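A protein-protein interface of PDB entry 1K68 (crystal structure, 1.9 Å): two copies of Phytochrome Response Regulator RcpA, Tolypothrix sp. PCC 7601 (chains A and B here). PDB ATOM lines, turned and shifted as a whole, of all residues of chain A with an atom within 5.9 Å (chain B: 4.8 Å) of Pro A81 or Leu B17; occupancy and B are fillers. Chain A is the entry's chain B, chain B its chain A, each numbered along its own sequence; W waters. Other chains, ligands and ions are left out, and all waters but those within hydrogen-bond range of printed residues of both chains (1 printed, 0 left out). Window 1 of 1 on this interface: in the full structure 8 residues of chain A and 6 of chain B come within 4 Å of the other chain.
The backbone NH of Leu A83 lies within hydrogen-bond range of the side-chain carboxylate of Asp A80, 3.4 Å away. NH1 of Arg A85 lies within hydrogen-bond range of O of Pro A81 (3.0 Å). The side-chain carboxylate (OD1) of Asp A80 is in hydrogen-bond range of the side-chain hydroxyl (OG1) of Thr A82. The backbone NH of Lys A84 is in hydrogen-bond range of the backbone carbonyl oxygen of Ile A77.
Water W1 lies within hydrogen-bond range of the backbone carbonyl oxygen (O) of Ser A79 (2.7 Å) and the backbone NH (N) of Ser B119 (3.1 Å).
No position is printed for both chains.
Printed residues of chain B within 4 Å of Thr A82: Glu B20. Of the printed residues of chain A, Leu B118 touches Pro A81 (3.5 Å). Leu A83 touches none of the printed residues of chain B. The nearest residue of chain B that does not touch Pro A81 is Ser B119 (4.05 Å). The nearest residue of chain A that does not touch Leu B17 is Thr A82 (4.6 Å). The nearest printed residue of chain B that does not touch Ser A79 is Leu B118 (4.1 Å).
Among the printed residues, pairs that only touch across the chains: Thr A82 with Glu B20, Pro A81 with Leu B118, Pro A81 with Phe B122, Pro A81 with Leu B17 and Lys A84 with Ser B119.
OD2 of Asp A80 is in salt-bridge range of NH2 of Arg B16 (3.1 Å). The side-chain hydroxyl (OG) of Ser B119 is in hydrogen-bond range of the backbone carbonyl oxygen (O) of Ser A79 (3.5 Å).
Printed residues of chain B that touch a printed residue of chain A: Arg B16, Leu B17, Glu B20, Leu B118, Ser B119 and Phe B122. Hydrophobic or aromatic side chains of chain B that line the printed part of chain A: Leu B17, Leu B118 and Phe B122.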
ATOM      1  N   ILE A  77      19.539   9.990 -18.686  1.00  0.00           N
ATOM      2  CA  ILE A  77      19.850   8.594 -18.418  1.00  0.00           C
ATOM      3  C   ILE A  77      19.439   8.200 -17.005  1.00  0.00           C
ATOM      4  O   ILE A  77      18.785   7.177 -16.795  1.00  0.00           O
ATOM      5  CB  ILE A  77      21.355   8.307 -18.549  1.00  0.00           C
ATOM      6  CG1 ILE A  77      21.774   8.386 -20.016  1.00  0.00           C
ATOM      7  CG2 ILE A  77      21.677   6.921 -17.963  1.00  0.00           C
ATOM      8  CD1 ILE A  77      23.231   8.070 -20.235  1.00  0.00           C
ATOM      9  N   SER A  79      17.281   9.474 -15.115  1.00  0.00           N
ATOM     10  CA  SER A  79      15.863   9.671 -14.827  1.00  0.00           C
ATOM     11  C   SER A  79      15.025   8.565 -15.449  1.00  0.00           C
ATOM     12  O   SER A  79      13.876   8.368 -15.081  1.00  0.00           O
ATOM     13  CB  SER A  79      15.391  11.017 -15.366  1.00  0.00           C
ATOM     14  OG  SER A  79      15.957  12.063 -14.610  1.00  0.00           O
ATOM     15  N   ASP A  80      15.612   7.848 -16.397  1.00  0.00           N
ATOM     16  CA  ASP A  80      14.909   6.769 -17.076  1.00  0.00           C
ATOM     17  C   ASP A  80      14.954   5.477 -16.263  1.00  0.00           C
ATOM     18  O   ASP A  80      16.033   4.947 -15.974  1.00  0.00           O
ATOM     19  CB  ASP A  80      15.519   6.546 -18.457  1.00  0.00           C
ATOM     20  CG  ASP A  80      14.665   5.665 -19.319  1.00  0.00           C
ATOM     21  OD1 ASP A  80      14.512   4.476 -18.971  1.00  0.00           O
ATOM     22  OD2 ASP A  80      14.140   6.167 -20.333  1.00  0.00           O
ATOM     23  N   PRO A  81      13.774   4.943 -15.892  1.00  0.00           N
ATOM     24  CA  PRO A  81      13.653   3.714 -15.101  1.00  0.00           C
ATOM     25  C   PRO A  81      14.262   2.463 -15.713  1.00  0.00           C
ATOM     26  O   PRO A  81      14.448   1.457 -15.023  1.00  0.00           O
ATOM     27  CB  PRO A  81      12.143   3.582 -14.899  1.00  0.00           C
ATOM     28  CG  PRO A  81      11.590   4.165 -16.147  1.00  0.00           C
ATOM     29  CD  PRO A  81      12.448   5.403 -16.341  1.00  0.00           C
ATOM     30  N   THR A  82      14.575   2.518 -17.001  1.00  0.00           N
ATOM     31  CA  THR A  82      15.166   1.369 -17.670  1.00  0.00           C
ATOM     32  C   THR A  82      16.663   1.554 -17.914  1.00  0.00           C
ATOM     33  O   THR A  82      17.364   0.593 -18.221  1.00  0.00           O
ATOM     34  CB  THR A  82      14.474   1.095 -19.026  1.00  0.00           C
ATOM     35  OG1 THR A  82      14.783   2.151 -19.948  1.00  0.00           O
ATOM     36  CG2 THR A  82      12.955   1.017 -18.846  1.00  0.00           C
ATOM     37  N   LEU A  83      17.158   2.781 -17.763  1.00  0.00           N
ATOM     38  CA  LEU A  83      18.574   3.063 -17.993  1.00  0.00           C
ATOM     39  C   LEU A  83      19.335   3.526 -16.749  1.00  0.00           C
ATOM     40  O   LEU A  83      20.559   3.416 -16.687  1.00  0.00           O
ATOM     41  CB  LEU A  83      18.711   4.150 -19.053  1.00  0.00           C
ATOM     42  CG  LEU A  83      17.951   3.948 -20.365  1.00  0.00           C
ATOM     43  CD1 LEU A  83      17.980   5.245 -21.152  1.00  0.00           C
ATOM     44  CD2 LEU A  83      18.576   2.801 -21.159  1.00  0.00           C
ATOM     45  N   LYS A  84      18.606   4.046 -15.772  1.00  0.00           N
ATOM     46  CA  LYS A  84      19.208   4.582 -14.556  1.00  0.00           C
ATOM     47  C   LYS A  84      20.120   3.652 -13.771  1.00  0.00           C
ATOM     48  O   LYS A  84      20.886   4.119 -12.930  1.00  0.00           O
ATOM     49  CB  LYS A  84      18.118   5.118 -13.631  1.00  0.00           C
ATOM     50  CG  LYS A  84      17.211   4.056 -13.039  1.00  0.00           C
ATOM     51  CD  LYS A  84      16.097   4.683 -12.204  1.00  0.00           C
ATOM     52  CE  LYS A  84      16.634   5.321 -10.934  1.00  0.00           C
ATOM     53  NZ  LYS A  84      15.560   5.924 -10.091  1.00  0.00           N
ATOM     54  N   ARG A  85      20.045   2.349 -14.030  1.00  0.00           N
ATOM     55  CA  ARG A  85      20.885   1.399 -13.311  1.00  0.00           C
ATOM     56  C   ARG A  85      22.211   1.116 -14.003  1.00  0.00           C
ATOM     57  O   ARG A  85      23.124   0.564 -13.393  1.00  0.00           O
ATOM     58  CB  ARG A  85      20.125   0.087 -13.065  1.00  0.00           C
ATOM     59  CG  ARG A  85      19.093   0.168 -11.940  1.00  0.00           C
ATOM     60  CD  ARG A  85      18.338  -1.150 -11.765  1.00  0.00           C
ATOM     61  NE  ARG A  85      17.657  -1.529 -13.002  1.00  0.00           N
ATOM     62  CZ  ARG A  85      16.672  -0.829 -13.556  1.00  0.00           C
ATOM     63  NH1 ARG A  85      16.239   0.282 -12.983  1.00  0.00           N
ATOM     64  NH2 ARG A  85      16.140  -1.226 -14.704  1.00  0.00           N
ATOM     65  N   ALA B  13       7.532   4.879 -26.781  1.00  0.00           N
ATOM     66  CA  ALA B  13       8.239   5.152 -25.538  1.00  0.00           C
ATOM     67  C   ALA B  13       7.536   4.436 -24.391  1.00  0.00           C
ATOM     68  O   ALA B  13       8.178   3.755 -23.590  1.00  0.00           O
ATOM     69  CB  ALA B  13       8.282   6.646 -25.275  1.00  0.00           C
ATOM     70  N   ASP B  14       6.217   4.601 -24.313  1.00  0.00           N
ATOM     71  CA  ASP B  14       5.434   3.965 -23.262  1.00  0.00           C
ATOM     72  C   ASP B  14       5.450   2.453 -23.432  1.00  0.00           C
ATOM     73  O   ASP B  14       5.514   1.712 -22.457  1.00  0.00           O
ATOM     74  CB  ASP B  14       3.983   4.465 -23.284  1.00  0.00           C
ATOM     75  CG  ASP B  14       3.860   5.925 -22.881  1.00  0.00           C
ATOM     76  OD1 ASP B  14       4.773   6.441 -22.203  1.00  0.00           O
ATOM     77  OD2 ASP B  14       2.845   6.560 -23.227  1.00  0.00           O
ATOM     78  N   ILE B  15       5.382   1.999 -24.678  1.00  0.00           N
ATOM     79  CA  ILE B  15       5.400   0.573 -24.942  1.00  0.00           C
ATOM     80  C   ILE B  15       6.675   0.000 -24.356  1.00  0.00           C
ATOM     81  O   ILE B  15       6.650  -1.028 -23.676  1.00  0.00           O
ATOM     82  CB  ILE B  15       5.352   0.276 -26.457  1.00  0.00           C
ATOM     83  CG1 ILE B  15       3.966   0.616 -27.005  1.00  0.00           C
ATOM     84  CG2 ILE B  15       5.679  -1.193 -26.709  1.00  0.00           C
ATOM     85  CD1 ILE B  15       3.842   0.492 -28.512  1.00  0.00           C
ATOM     86  N   ARG B  16       7.791   0.676 -24.613  1.00  0.00           N
ATOM     87  CA  ARG B  16       9.075   0.214 -24.110  1.00  0.00           C
ATOM     88  C   ARG B  16       9.054   0.112 -22.593  1.00  0.00           C
ATOM     89  O   ARG B  16       9.323  -0.953 -22.032  1.00  0.00           O
ATOM     90  CB  ARG B  16      10.213   1.153 -24.535  1.00  0.00           C
ATOM     91  CG  ARG B  16      11.588   0.638 -24.123  1.00  0.00           C
ATOM     92  CD  ARG B  16      12.743   1.536 -24.572  1.00  0.00           C
ATOM     93  NE  ARG B  16      13.053   2.601 -23.616  1.00  0.00           N
ATOM     94  CZ  ARG B  16      12.610   3.853 -23.711  1.00  0.00           C
ATOM     95  NH1 ARG B  16      11.832   4.215 -24.726  1.00  0.00           N
ATOM     96  NH2 ARG B  16      12.948   4.746 -22.789  1.00  0.00           N
ATOM     97  N   LEU B  17       8.722   1.219 -21.937  1.00  0.00           N
ATOM     98  CA  LEU B  17       8.685   1.272 -20.481  1.00  0.00           C
ATOM     99  C   LEU B  17       7.740   0.225 -19.885  1.00  0.00           C
ATOM    100  O   LEU B  17       8.114  -0.523 -18.979  1.00  0.00           O
ATOM    101  CB  LEU B  17       8.283   2.680 -20.040  1.00  0.00           C
ATOM    102  CG  LEU B  17       8.355   3.014 -18.547  1.00  0.00           C
ATOM    103  CD1 LEU B  17       8.464   4.518 -18.379  1.00  0.00           C
ATOM    104  CD2 LEU B  17       7.135   2.467 -17.819  1.00  0.00           C
ATOM    105  N   ILE B  18       6.517   0.171 -20.398  1.00  0.00           N
ATOM    106  CA  ILE B  18       5.542  -0.798 -19.921  1.00  0.00           C
ATOM    107  C   ILE B  18       6.084  -2.218 -20.063  1.00  0.00           C
ATOM    108  O   ILE B  18       5.963  -3.025 -19.143  1.00  0.00           O
ATOM    109  CB  ILE B  18       4.209  -0.659 -20.695  1.00  0.00           C
ATOM    110  CG1 ILE B  18       3.588   0.707 -20.393  1.00  0.00           C
ATOM    111  CG2 ILE B  18       3.252  -1.774 -20.298  1.00  0.00           C
ATOM    112  CD1 ILE B  18       2.310   1.003 -21.164  1.00  0.00           C
ATOM    113  N   GLN B  19       6.684  -2.528 -21.212  1.00  0.00           N
ATOM    114  CA  GLN B  19       7.249  -3.860 -21.423  1.00  0.00           C
ATOM    115  C   GLN B  19       8.410  -4.144 -20.470  1.00  0.00           C
ATOM    116  O   GLN B  19       8.607  -5.285 -20.048  1.00  0.00           O
ATOM    117  CB  GLN B  19       7.725  -4.027 -22.868  1.00  0.00           C
ATOM    118  CG  GLN B  19       6.591  -4.027 -23.875  1.00  0.00           C
ATOM    119  CD  GLN B  19       7.058  -4.332 -25.282  1.00  0.00           C
ATOM    120  OE1 GLN B  19       8.113  -3.864 -25.714  1.00  0.00           O
ATOM    121  NE2 GLN B  19       6.265  -5.104 -26.013  1.00  0.00           N
ATOM    122  N   GLU B  20       9.169  -3.108 -20.130  1.00  0.00           N
ATOM    123  CA  GLU B  20      10.303  -3.253 -19.217  1.00  0.00           C
ATOM    124  C   GLU B  20       9.833  -3.514 -17.794  1.00  0.00           C
ATOM    125  O   GLU B  20      10.401  -4.346 -17.080  1.00  0.00           O
ATOM    126  CB  GLU B  20      11.164  -1.991 -19.224  1.00  0.00           C
ATOM    127  CG  GLU B  20      11.864  -1.737 -20.534  1.00  0.00           C
ATOM    128  CD  GLU B  20      12.706  -2.913 -20.948  1.00  0.00           C
ATOM    129  OE1 GLU B  20      13.543  -3.343 -20.127  1.00  0.00           O
ATOM    130  OE2 GLU B  20      12.529  -3.408 -22.082  1.00  0.00           O
ATOM    131  N   ALA B  21       8.798  -2.794 -17.382  1.00  0.00           N
ATOM    132  CA  ALA B  21       8.263  -2.953 -16.042  1.00  0.00           C
ATOM    133  C   ALA B  21       7.653  -4.340 -15.870  1.00  0.00           C
ATOM    134  O   ALA B  21       7.872  -5.000 -14.855  1.00  0.00           O
ATOM    135  CB  ALA B  21       7.225  -1.877 -15.765  1.00  0.00           C
ATOM    136  N   LEU B 118       8.653   9.324 -15.390  1.00  0.00           N
ATOM    137  CA  LEU B 118       8.905   7.974 -15.881  1.00  0.00           C
ATOM    138  C   LEU B 118       9.062   6.933 -14.779  1.00  0.00           C
ATOM    139  O   LEU B 118       8.448   5.868 -14.844  1.00  0.00           O
ATOM    140  CB  LEU B 118      10.148   7.963 -16.777  1.00  0.00           C
ATOM    141  CG  LEU B 118      10.071   8.751 -18.091  1.00  0.00           C
ATOM    142  CD1 LEU B 118      11.434   8.808 -18.737  1.00  0.00           C
ATOM    143  CD2 LEU B 118       9.077   8.093 -19.032  1.00  0.00           C
ATOM    144  N   SER B 119       9.871   7.230 -13.765  1.00  0.00           N
ATOM    145  CA  SER B 119      10.079   6.271 -12.686  1.00  0.00           C
ATOM    146  C   SER B 119       8.776   5.990 -11.942  1.00  0.00           C
ATOM    147  O   SER B 119       8.523   4.857 -11.521  1.00  0.00           O
ATOM    148  CB  SER B 119      11.162   6.773 -11.718  1.00  0.00           C
ATOM    149  OG  SER B 119      12.438   6.766 -12.345  1.00  0.00           O
ATOM    150  N   LEU B 121       5.735   6.192 -13.259  1.00  0.00           N
ATOM    151  CA  LEU B 121       4.941   5.376 -14.171  1.00  0.00           C
ATOM    152  C   LEU B 121       5.452   3.940 -14.122  1.00  0.00           C
ATOM    153  O   LEU B 121       4.669   2.992 -14.112  1.00  0.00           O
ATOM    154  CB  LEU B 121       5.048   5.925 -15.591  1.00  0.00           C
ATOM    155  CG  LEU B 121       4.383   5.123 -16.711  1.00  0.00           C
ATOM    156  CD1 LEU B 121       2.887   4.975 -16.459  1.00  0.00           C
ATOM    157  CD2 LEU B 121       4.630   5.835 -18.019  1.00  0.00           C
ATOM    158  N   PHE B 122       6.772   3.784 -14.089  1.00  0.00           N
ATOM    159  CA  PHE B 122       7.358   2.454 -14.026  1.00  0.00           C
ATOM    160  C   PHE B 122       6.820   1.741 -12.787  1.00  0.00           C
ATOM    161  O   PHE B 122       6.441   0.578 -12.846  1.00  0.00           O
ATOM    162  CB  PHE B 122       8.882   2.546 -13.950  1.00  0.00           C
ATOM    163  CG  PHE B 122       9.585   1.228 -14.147  1.00  0.00           C
ATOM    164  CD1 PHE B 122       9.915   0.787 -15.425  1.00  0.00           C
ATOM    165  CD2 PHE B 122       9.915   0.431 -13.058  1.00  0.00           C
ATOM    166  CE1 PHE B 122      10.574  -0.428 -15.616  1.00  0.00           C
ATOM    167  CE2 PHE B 122      10.570  -0.787 -13.232  1.00  0.00           C
ATOM    168  CZ  PHE B 122      10.900  -1.217 -14.516  1.00  0.00           C
ATOM    169  N   VAL B 125       3.150   0.658 -13.247  1.00  0.00           N
ATOM    170  CA  VAL B 125       2.974  -0.566 -14.014  1.00  0.00           C
ATOM    171  C   VAL B 125       3.285  -1.761 -13.127  1.00  0.00           C
ATOM    172  O   VAL B 125       2.625  -2.796 -13.217  1.00  0.00           O
ATOM    173  CB  VAL B 125       3.878  -0.591 -15.259  1.00  0.00           C
ATOM    174  CG1 VAL B 125       3.730  -1.928 -15.991  1.00  0.00           C
ATOM    175  CG2 VAL B 125       3.506   0.562 -16.184  1.00  0.00           C
HETATM  176  O   HOH W   1      11.810   9.626 -13.876  1.00  0.00           O
